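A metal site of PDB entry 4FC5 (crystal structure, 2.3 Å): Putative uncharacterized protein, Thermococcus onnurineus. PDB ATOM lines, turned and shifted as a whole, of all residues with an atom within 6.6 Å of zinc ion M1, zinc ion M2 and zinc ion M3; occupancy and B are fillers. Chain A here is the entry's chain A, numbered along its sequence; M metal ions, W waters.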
ATOM      1  N   PHE A  50      10.093 -13.188  21.578  1.00  0.00           N
ATOM      2  CA  PHE A  50       9.051 -12.754  22.493  1.00  0.00           C
ATOM      3  C   PHE A  50       9.520 -12.812  23.941  1.00  0.00           C
ATOM      4  O   PHE A  50       9.599 -13.877  24.542  1.00  0.00           O
ATOM      5  CB  PHE A  50       7.792 -13.613  22.333  1.00  0.00           C
ATOM      6  CG  PHE A  50       6.532 -12.886  22.640  1.00  0.00           C
ATOM      7  CD1 PHE A  50       5.744 -12.385  21.608  1.00  0.00           C
ATOM      8  CD2 PHE A  50       6.153 -12.654  23.953  1.00  0.00           C
ATOM      9  CE1 PHE A  50       4.593 -11.669  21.884  1.00  0.00           C
ATOM     10  CE2 PHE A  50       4.993 -11.931  24.238  1.00  0.00           C
ATOM     11  CZ  PHE A  50       4.212 -11.445  23.201  1.00  0.00           C
ATOM     12  N   ILE A  52       9.598 -12.861  27.847  1.00  0.00           N
ATOM     13  CA  ILE A  52       8.622 -13.370  28.793  1.00  0.00           C
ATOM     14  C   ILE A  52       8.829 -12.837  30.200  1.00  0.00           C
ATOM     15  O   ILE A  52       9.871 -13.070  30.801  1.00  0.00           O
ATOM     16  CB  ILE A  52       8.660 -14.900  28.767  1.00  0.00           C
ATOM     17  CG1 ILE A  52       8.133 -15.361  27.422  1.00  0.00           C
ATOM     18  CG2 ILE A  52       7.849 -15.498  29.917  1.00  0.00           C
ATOM     19  CD1 ILE A  52       8.139 -16.807  27.221  1.00  0.00           C
ATOM     20  N   GLU A  59      11.464 -16.645  24.167  1.00  0.00           N
ATOM     21  CA  GLU A  59      11.030 -18.014  24.303  1.00  0.00           C
ATOM     22  C   GLU A  59      11.338 -18.832  23.074  1.00  0.00           C
ATOM     23  O   GLU A  59      11.830 -18.291  22.086  1.00  0.00           O
ATOM     24  CB  GLU A  59       9.520 -18.056  24.596  1.00  0.00           C
ATOM     25  CG  GLU A  59       8.658 -17.443  23.517  1.00  0.00           C
ATOM     26  CD  GLU A  59       7.177 -17.691  23.708  1.00  0.00           C
ATOM     27  OE1 GLU A  59       6.459 -16.746  24.091  1.00  0.00           O
ATOM     28  OE2 GLU A  59       6.728 -18.834  23.471  1.00  0.00           O
ATOM     29  N   THR A  60      11.036 -20.131  23.145  1.00  0.00           N
ATOM     30  CA  THR A  60      11.267 -21.072  22.045  1.00  0.00           C
ATOM     31  C   THR A  60      10.214 -21.058  20.924  1.00  0.00           C
ATOM     32  O   THR A  60      10.401 -21.695  19.890  1.00  0.00           O
ATOM     33  CB  THR A  60      11.388 -22.505  22.591  1.00  0.00           C
ATOM     34  OG1 THR A  60      10.512 -22.665  23.708  1.00  0.00           O
ATOM     35  CG2 THR A  60      12.819 -22.797  23.023  1.00  0.00           C
ATOM     36  N   ASP A  61       9.107 -20.364  21.126  1.00  0.00           N
ATOM     37  CA  ASP A  61       8.122 -20.274  20.060  1.00  0.00           C
ATOM     38  C   ASP A  61       8.530 -19.060  19.260  1.00  0.00           C
ATOM     39  O   ASP A  61       8.739 -17.981  19.845  1.00  0.00           O
ATOM     40  CB  ASP A  61       6.723 -20.039  20.604  1.00  0.00           C
ATOM     41  CG  ASP A  61       5.659 -20.220  19.562  1.00  0.00           C
ATOM     42  OD1 ASP A  61       4.504 -19.804  19.810  1.00  0.00           O
ATOM     43  OD2 ASP A  61       5.949 -20.782  18.486  1.00  0.00           O
ATOM     44  N   GLY A  62       8.648 -19.218  17.944  1.00  0.00           N
ATOM     45  CA  GLY A  62       9.044 -18.112  17.088  1.00  0.00           C
ATOM     46  C   GLY A  62      10.356 -18.331  16.355  1.00  0.00           C
ATOM     47  O   GLY A  62      10.376 -18.438  15.129  1.00  0.00           O
ATOM     48  N   GLU A 115       5.797 -14.637  15.954  1.00  0.00           N
ATOM     49  CA  GLU A 115       5.767 -14.473  17.413  1.00  0.00           C
ATOM     50  C   GLU A 115       6.619 -13.298  17.874  1.00  0.00           C
ATOM     51  O   GLU A 115       7.735 -13.484  18.349  1.00  0.00           O
ATOM     52  CB  GLU A 115       6.249 -15.753  18.115  1.00  0.00           C
ATOM     53  CG  GLU A 115       5.771 -15.869  19.562  1.00  0.00           C
ATOM     54  CD  GLU A 115       4.269 -15.938  19.676  1.00  0.00           C
ATOM     55  OE1 GLU A 115       3.593 -15.885  18.631  1.00  0.00           O
ATOM     56  OE2 GLU A 115       3.756 -16.059  20.802  1.00  0.00           O
ATOM     57  N   MET A 128       0.705 -13.143  27.506  1.00  0.00           N
ATOM     58  CA  MET A 128      -0.614 -13.768  27.596  1.00  0.00           C
ATOM     59  C   MET A 128      -1.232 -13.578  28.974  1.00  0.00           C
ATOM     60  O   MET A 128      -2.455 -13.628  29.120  1.00  0.00           O
ATOM     61  CB  MET A 128      -0.552 -15.259  27.242  1.00  0.00           C
ATOM     62  CG  MET A 128      -0.333 -15.557  25.758  1.00  0.00           C
ATOM     63  SD  MET A 128      -1.317 -14.532  24.621  1.00  0.00           S
ATOM     64  CE  MET A 128      -2.959 -15.221  24.776  1.00  0.00           C
ATOM     65  N   GLY A 156       0.965 -15.383  14.545  1.00  0.00           N
ATOM     66  CA  GLY A 156       0.730 -15.392  15.984  1.00  0.00           C
ATOM     67  C   GLY A 156      -0.234 -16.496  16.395  1.00  0.00           C
ATOM     68  O   GLY A 156      -0.880 -17.116  15.555  1.00  0.00           O
ATOM     69  N   ASP A 157      -0.359 -16.710  17.698  1.00  0.00           N
ATOM     70  CA  ASP A 157      -1.228 -17.761  18.217  1.00  0.00           C
ATOM     71  C   ASP A 157      -1.951 -17.332  19.475  1.00  0.00           C
ATOM     72  O   ASP A 157      -2.539 -18.166  20.162  1.00  0.00           O
ATOM     73  CB  ASP A 157      -0.379 -19.001  18.544  1.00  0.00           C
ATOM     74  CG  ASP A 157       0.776 -18.684  19.481  1.00  0.00           C
ATOM     75  OD1 ASP A 157       1.014 -17.485  19.763  1.00  0.00           O
ATOM     76  OD2 ASP A 157       1.459 -19.628  19.928  1.00  0.00           O
ATOM     77  N   GLY A 158      -1.918 -16.041  19.783  1.00  0.00           N
ATOM     78  CA  GLY A 158      -2.576 -15.575  20.980  1.00  0.00           C
ATOM     79  C   GLY A 158      -3.318 -14.253  20.902  1.00  0.00           C
ATOM     80  O   GLY A 158      -4.338 -14.088  21.555  1.00  0.00           O
ATOM     81  N   GLY A 159      -2.804 -13.303  20.132  1.00  0.00           N
ATOM     82  CA  GLY A 159      -3.506 -12.038  20.022  1.00  0.00           C
ATOM     83  C   GLY A 159      -2.709 -10.814  20.431  1.00  0.00           C
ATOM     84  O   GLY A 159      -3.181  -9.682  20.312  1.00  0.00           O
ATOM     85  N   ASN A 160      -1.503 -11.015  20.925  1.00  0.00           N
ATOM     86  CA  ASN A 160      -0.706  -9.900  21.322  1.00  0.00           C
ATOM     87  C   ASN A 160       0.551  -9.830  20.449  1.00  0.00           C
ATOM     88  O   ASN A 160       1.523  -9.205  20.813  1.00  0.00           O
ATOM     89  CB  ASN A 160      -0.335 -10.057  22.789  1.00  0.00           C
ATOM     90  CG  ASN A 160       0.424 -11.328  23.054  1.00  0.00           C
ATOM     91  OD1 ASN A 160       0.394 -12.258  22.243  1.00  0.00           O
ATOM     92  ND2 ASN A 160       1.102 -11.389  24.192  1.00  0.00           N
ATOM     93  N   GLU A 161       0.503 -10.496  19.292  1.00  0.00           N
ATOM     94  CA  GLU A 161       1.629 -10.517  18.359  1.00  0.00           C
ATOM     95  C   GLU A 161       1.444  -9.568  17.186  1.00  0.00           C
ATOM     96  O   GLU A 161       0.332  -9.268  16.799  1.00  0.00           O
ATOM     97  CB  GLU A 161       1.849 -11.936  17.821  1.00  0.00           C
ATOM     98  CG  GLU A 161       2.089 -12.997  18.863  1.00  0.00           C
ATOM     99  CD  GLU A 161       0.811 -13.654  19.337  1.00  0.00           C
ATOM    100  OE1 GLU A 161      -0.260 -12.998  19.350  1.00  0.00           O
ATOM    101  OE2 GLU A 161       0.867 -14.846  19.713  1.00  0.00           O
ATOM    102  N   MET A 164      -1.731  -9.237  14.573  1.00  0.00           N
ATOM    103  CA  MET A 164      -2.988  -9.598  15.221  1.00  0.00           C
ATOM    104  C   MET A 164      -3.913  -8.384  15.359  1.00  0.00           C
ATOM    105  O   MET A 164      -5.064  -8.496  15.775  1.00  0.00           O
ATOM    106  CB  MET A 164      -2.677 -10.178  16.607  1.00  0.00           C
ATOM    107  CG  MET A 164      -3.625 -11.262  17.085  1.00  0.00           C
ATOM    108  SD  MET A 164      -3.528 -12.833  16.224  1.00  0.00           S
ATOM    109  CE  MET A 164      -2.254 -13.652  17.103  1.00  0.00           C
ATOM    110  N   ALA A 194      -2.241 -22.608  16.374  1.00  0.00           N
ATOM    111  CA  ALA A 194      -2.146 -22.936  17.807  1.00  0.00           C
ATOM    112  C   ALA A 194      -0.790 -22.599  18.368  1.00  0.00           C
ATOM    113  O   ALA A 194      -0.673 -22.227  19.531  1.00  0.00           O
ATOM    114  CB  ALA A 194      -2.426 -24.430  18.032  1.00  0.00           C
ATOM    115  N   VAL A 195       0.224 -22.748  17.527  1.00  0.00           N
ATOM    116  CA  VAL A 195       1.614 -22.462  17.894  1.00  0.00           C
ATOM    117  C   VAL A 195       2.235 -21.776  16.702  1.00  0.00           C
ATOM    118  O   VAL A 195       2.268 -22.351  15.611  1.00  0.00           O
ATOM    119  CB  VAL A 195       2.396 -23.774  18.154  1.00  0.00           C
ATOM    120  CG1 VAL A 195       3.863 -23.465  18.352  1.00  0.00           C
ATOM    121  CG2 VAL A 195       1.811 -24.488  19.367  1.00  0.00           C
ATOM    122  N   SER A 196       2.758 -20.562  16.904  1.00  0.00           N
ATOM    123  CA  SER A 196       3.338 -19.785  15.807  1.00  0.00           C
ATOM    124  C   SER A 196       4.303 -20.544  14.922  1.00  0.00           C
ATOM    125  O   SER A 196       4.200 -20.484  13.695  1.00  0.00           O
ATOM    126  CB  SER A 196       3.997 -18.514  16.346  1.00  0.00           C
ATOM    127  OG  SER A 196       3.044 -17.698  17.019  1.00  0.00           O
ATOM    128  N   ASN A 197       5.234 -21.276  15.521  1.00  0.00           N
ATOM    129  CA  ASN A 197       6.191 -22.041  14.731  1.00  0.00           C
ATOM    130  C   ASN A 197       5.446 -22.812  13.642  1.00  0.00           C
ATOM    131  O   ASN A 197       5.837 -22.793  12.482  1.00  0.00           O
ATOM    132  CB  ASN A 197       6.968 -23.020  15.613  1.00  0.00           C
ATOM    133  CG  ASN A 197       7.938 -22.324  16.562  1.00  0.00           C
ATOM    134  OD1 ASN A 197       8.265 -22.851  17.625  1.00  0.00           O
ATOM    135  ND2 ASN A 197       8.409 -21.144  16.190  1.00  0.00           N
ATOM    136  N   ASP A 235      10.817 -21.926  27.700  1.00  0.00           N
ATOM    137  CA  ASP A 235       9.493 -22.356  27.318  1.00  0.00           C
ATOM    138  C   ASP A 235       8.587 -21.242  27.832  1.00  0.00           C
ATOM    139  O   ASP A 235       8.676 -20.856  28.992  1.00  0.00           O
ATOM    140  CB  ASP A 235       9.133 -23.672  28.005  1.00  0.00           C
ATOM    141  CG  ASP A 235       7.707 -24.076  27.749  1.00  0.00           C
ATOM    142  OD1 ASP A 235       7.430 -24.748  26.727  1.00  0.00           O
ATOM    143  OD2 ASP A 235       6.854 -23.701  28.588  1.00  0.00           O
ATOM    144  N   GLY A 236       7.728 -20.720  26.969  1.00  0.00           N
ATOM    145  CA  GLY A 236       6.853 -19.632  27.357  1.00  0.00           C
ATOM    146  C   GLY A 236       5.854 -19.907  28.458  1.00  0.00           C
ATOM    147  O   GLY A 236       5.461 -18.985  29.171  1.00  0.00           O
ATOM    148  N   VAL A 237       5.441 -21.162  28.601  1.00  0.00           N
ATOM    149  CA  VAL A 237       4.467 -21.506  29.621  1.00  0.00           C
ATOM    150  C   VAL A 237       5.114 -21.903  30.958  1.00  0.00           C
ATOM    151  O   VAL A 237       4.705 -21.434  32.018  1.00  0.00           O
ATOM    152  CB  VAL A 237       3.541 -22.637  29.136  1.00  0.00           C
ATOM    153  CG1 VAL A 237       2.801 -23.238  30.302  1.00  0.00           C
ATOM    154  CG2 VAL A 237       2.550 -22.081  28.126  1.00  0.00           C
ATOM    155  N   VAL A 245       7.954 -26.071  23.407  1.00  0.00           N
ATOM    156  CA  VAL A 245       7.482 -24.754  23.013  1.00  0.00           C
ATOM    157  C   VAL A 245       6.026 -24.644  23.436  1.00  0.00           C
ATOM    158  O   VAL A 245       5.223 -25.528  23.148  1.00  0.00           O
ATOM    159  CB  VAL A 245       7.693 -24.520  21.496  1.00  0.00           C
ATOM    160  CG1 VAL A 245       7.887 -25.819  20.788  1.00  0.00           C
ATOM    161  CG2 VAL A 245       6.532 -23.770  20.907  1.00  0.00           C
ATOM    162  N   ASP A 246       5.709 -23.577  24.143  1.00  0.00           N
ATOM    163  CA  ASP A 246       4.374 -23.318  24.644  1.00  0.00           C
ATOM    164  C   ASP A 246       3.819 -24.497  25.423  1.00  0.00           C
ATOM    165  O   ASP A 246       2.644 -24.834  25.302  1.00  0.00           O
ATOM    166  CB  ASP A 246       3.420 -22.976  23.501  1.00  0.00           C
ATOM    167  CG  ASP A 246       3.812 -21.702  22.786  1.00  0.00           C
ATOM    168  OD1 ASP A 246       4.543 -20.889  23.369  1.00  0.00           O
ATOM    169  OD2 ASP A 246       3.370 -21.511  21.639  1.00  0.00           O
HETATM  170 ZN    ZN M   1       1.760 -15.884  21.186  1.00  0.00          ZN
HETATM  171 ZN    ZN M   2       3.267 -19.410  21.088  1.00  0.00          ZN
HETATM  172 ZN    ZN M   3       4.725 -18.837  23.754  1.00  0.00          ZN
HETATM  173  O   HOH W   1       0.476 -17.962  22.489  1.00  0.00           O
HETATM  174  O   HOH W   2       3.398 -18.611  25.763  1.00  0.00           O
HETATM  175  O   HOH W   3       2.660 -14.518  22.663  1.00  0.00           O
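OD1 of Asp 61 sits close to N of Ser 196 (3.5 Å).
The side-chain carboxylate (OE1) of Glu 161 lies within hydrogen-bond range of the backbone NH (N) of Gly 158 (3.5 Å).
The backbone carbonyl oxygen (O) of Phe 50 is in hydrogen-bond range of the backbone NH (N) of Glu 59, 3.4 Å away.
The side-chain carboxylate (OE1) of Glu 115 sits at hydrogen-bond distance from the side-chain hydroxyl (OG) of Ser 196, at 2.5 Å.
OD1 of Asn 160 sits close to OE1 of Glu 161, 3.1 Å away.
The side-chain hydroxyl (OG) of Ser 196 lies close to the side-chain carboxylate (OD1) of Asp 157, 3.4 Å away.
The side-chain carboxylate of Asp 61 lies within hydrogen-bond range of the backbone NH of Asn 197, at 3.1 Å.
OE1 of Glu 161 lies within hydrogen-bond range of N of Gly 159 (2.7 Å).
Residues that only touch zinc ion M1: Gly 158 (3.9 Å).
The nearest printed residue that does not touch zinc ion M1 is Asn 160 (4.02 Å).
Within 4 Å of zinc ion M2: Asp 61, Glu 115, Asp 157 and Asp 246.
Three residues have an atom within 4 Å of zinc ion M3: Glu 59, Asp 61 and Asp 246.
The nearest printed residue that does not touch zinc ion M3 is Glu 115 (4.2 Å).
Zinc ion M1 is bound by the side-chain carboxylate (OE2) of Glu 161 (2.0 Å), the side-chain carboxylate (OE2) of Glu 115 (2.0 Å), water W3 (2.2 Å) and the side-chain carboxylate (OD1) of Asp 157 (2.3 Å).
Zinc ion M1 has four donor atoms within binding distance.
Slightly farther from zinc ion M1 lies water W1 (2.8 Å).
Zinc ion M2 is bound by the side-chain carboxylate (OD1) of Asp 61, 1.8 Å away.
Zinc ion M2 is bound by OD2 of Asp 157, 2.2 Å away.
Zinc ion M2 is bound by OD2 of Asp 246, 2.2 Å away.
Zinc ion M3 is bound by OE2 of Glu 59 (2.0 Å), OD1 of Asp 246 (2.1 Å) and water W2 (2.4 Å).
Zinc ion M3 has three donor atoms within binding distance.
Slightly farther from zinc ion M3 lies the side-chain carboxylate (OE1) of Glu 59 (2.7 Å).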
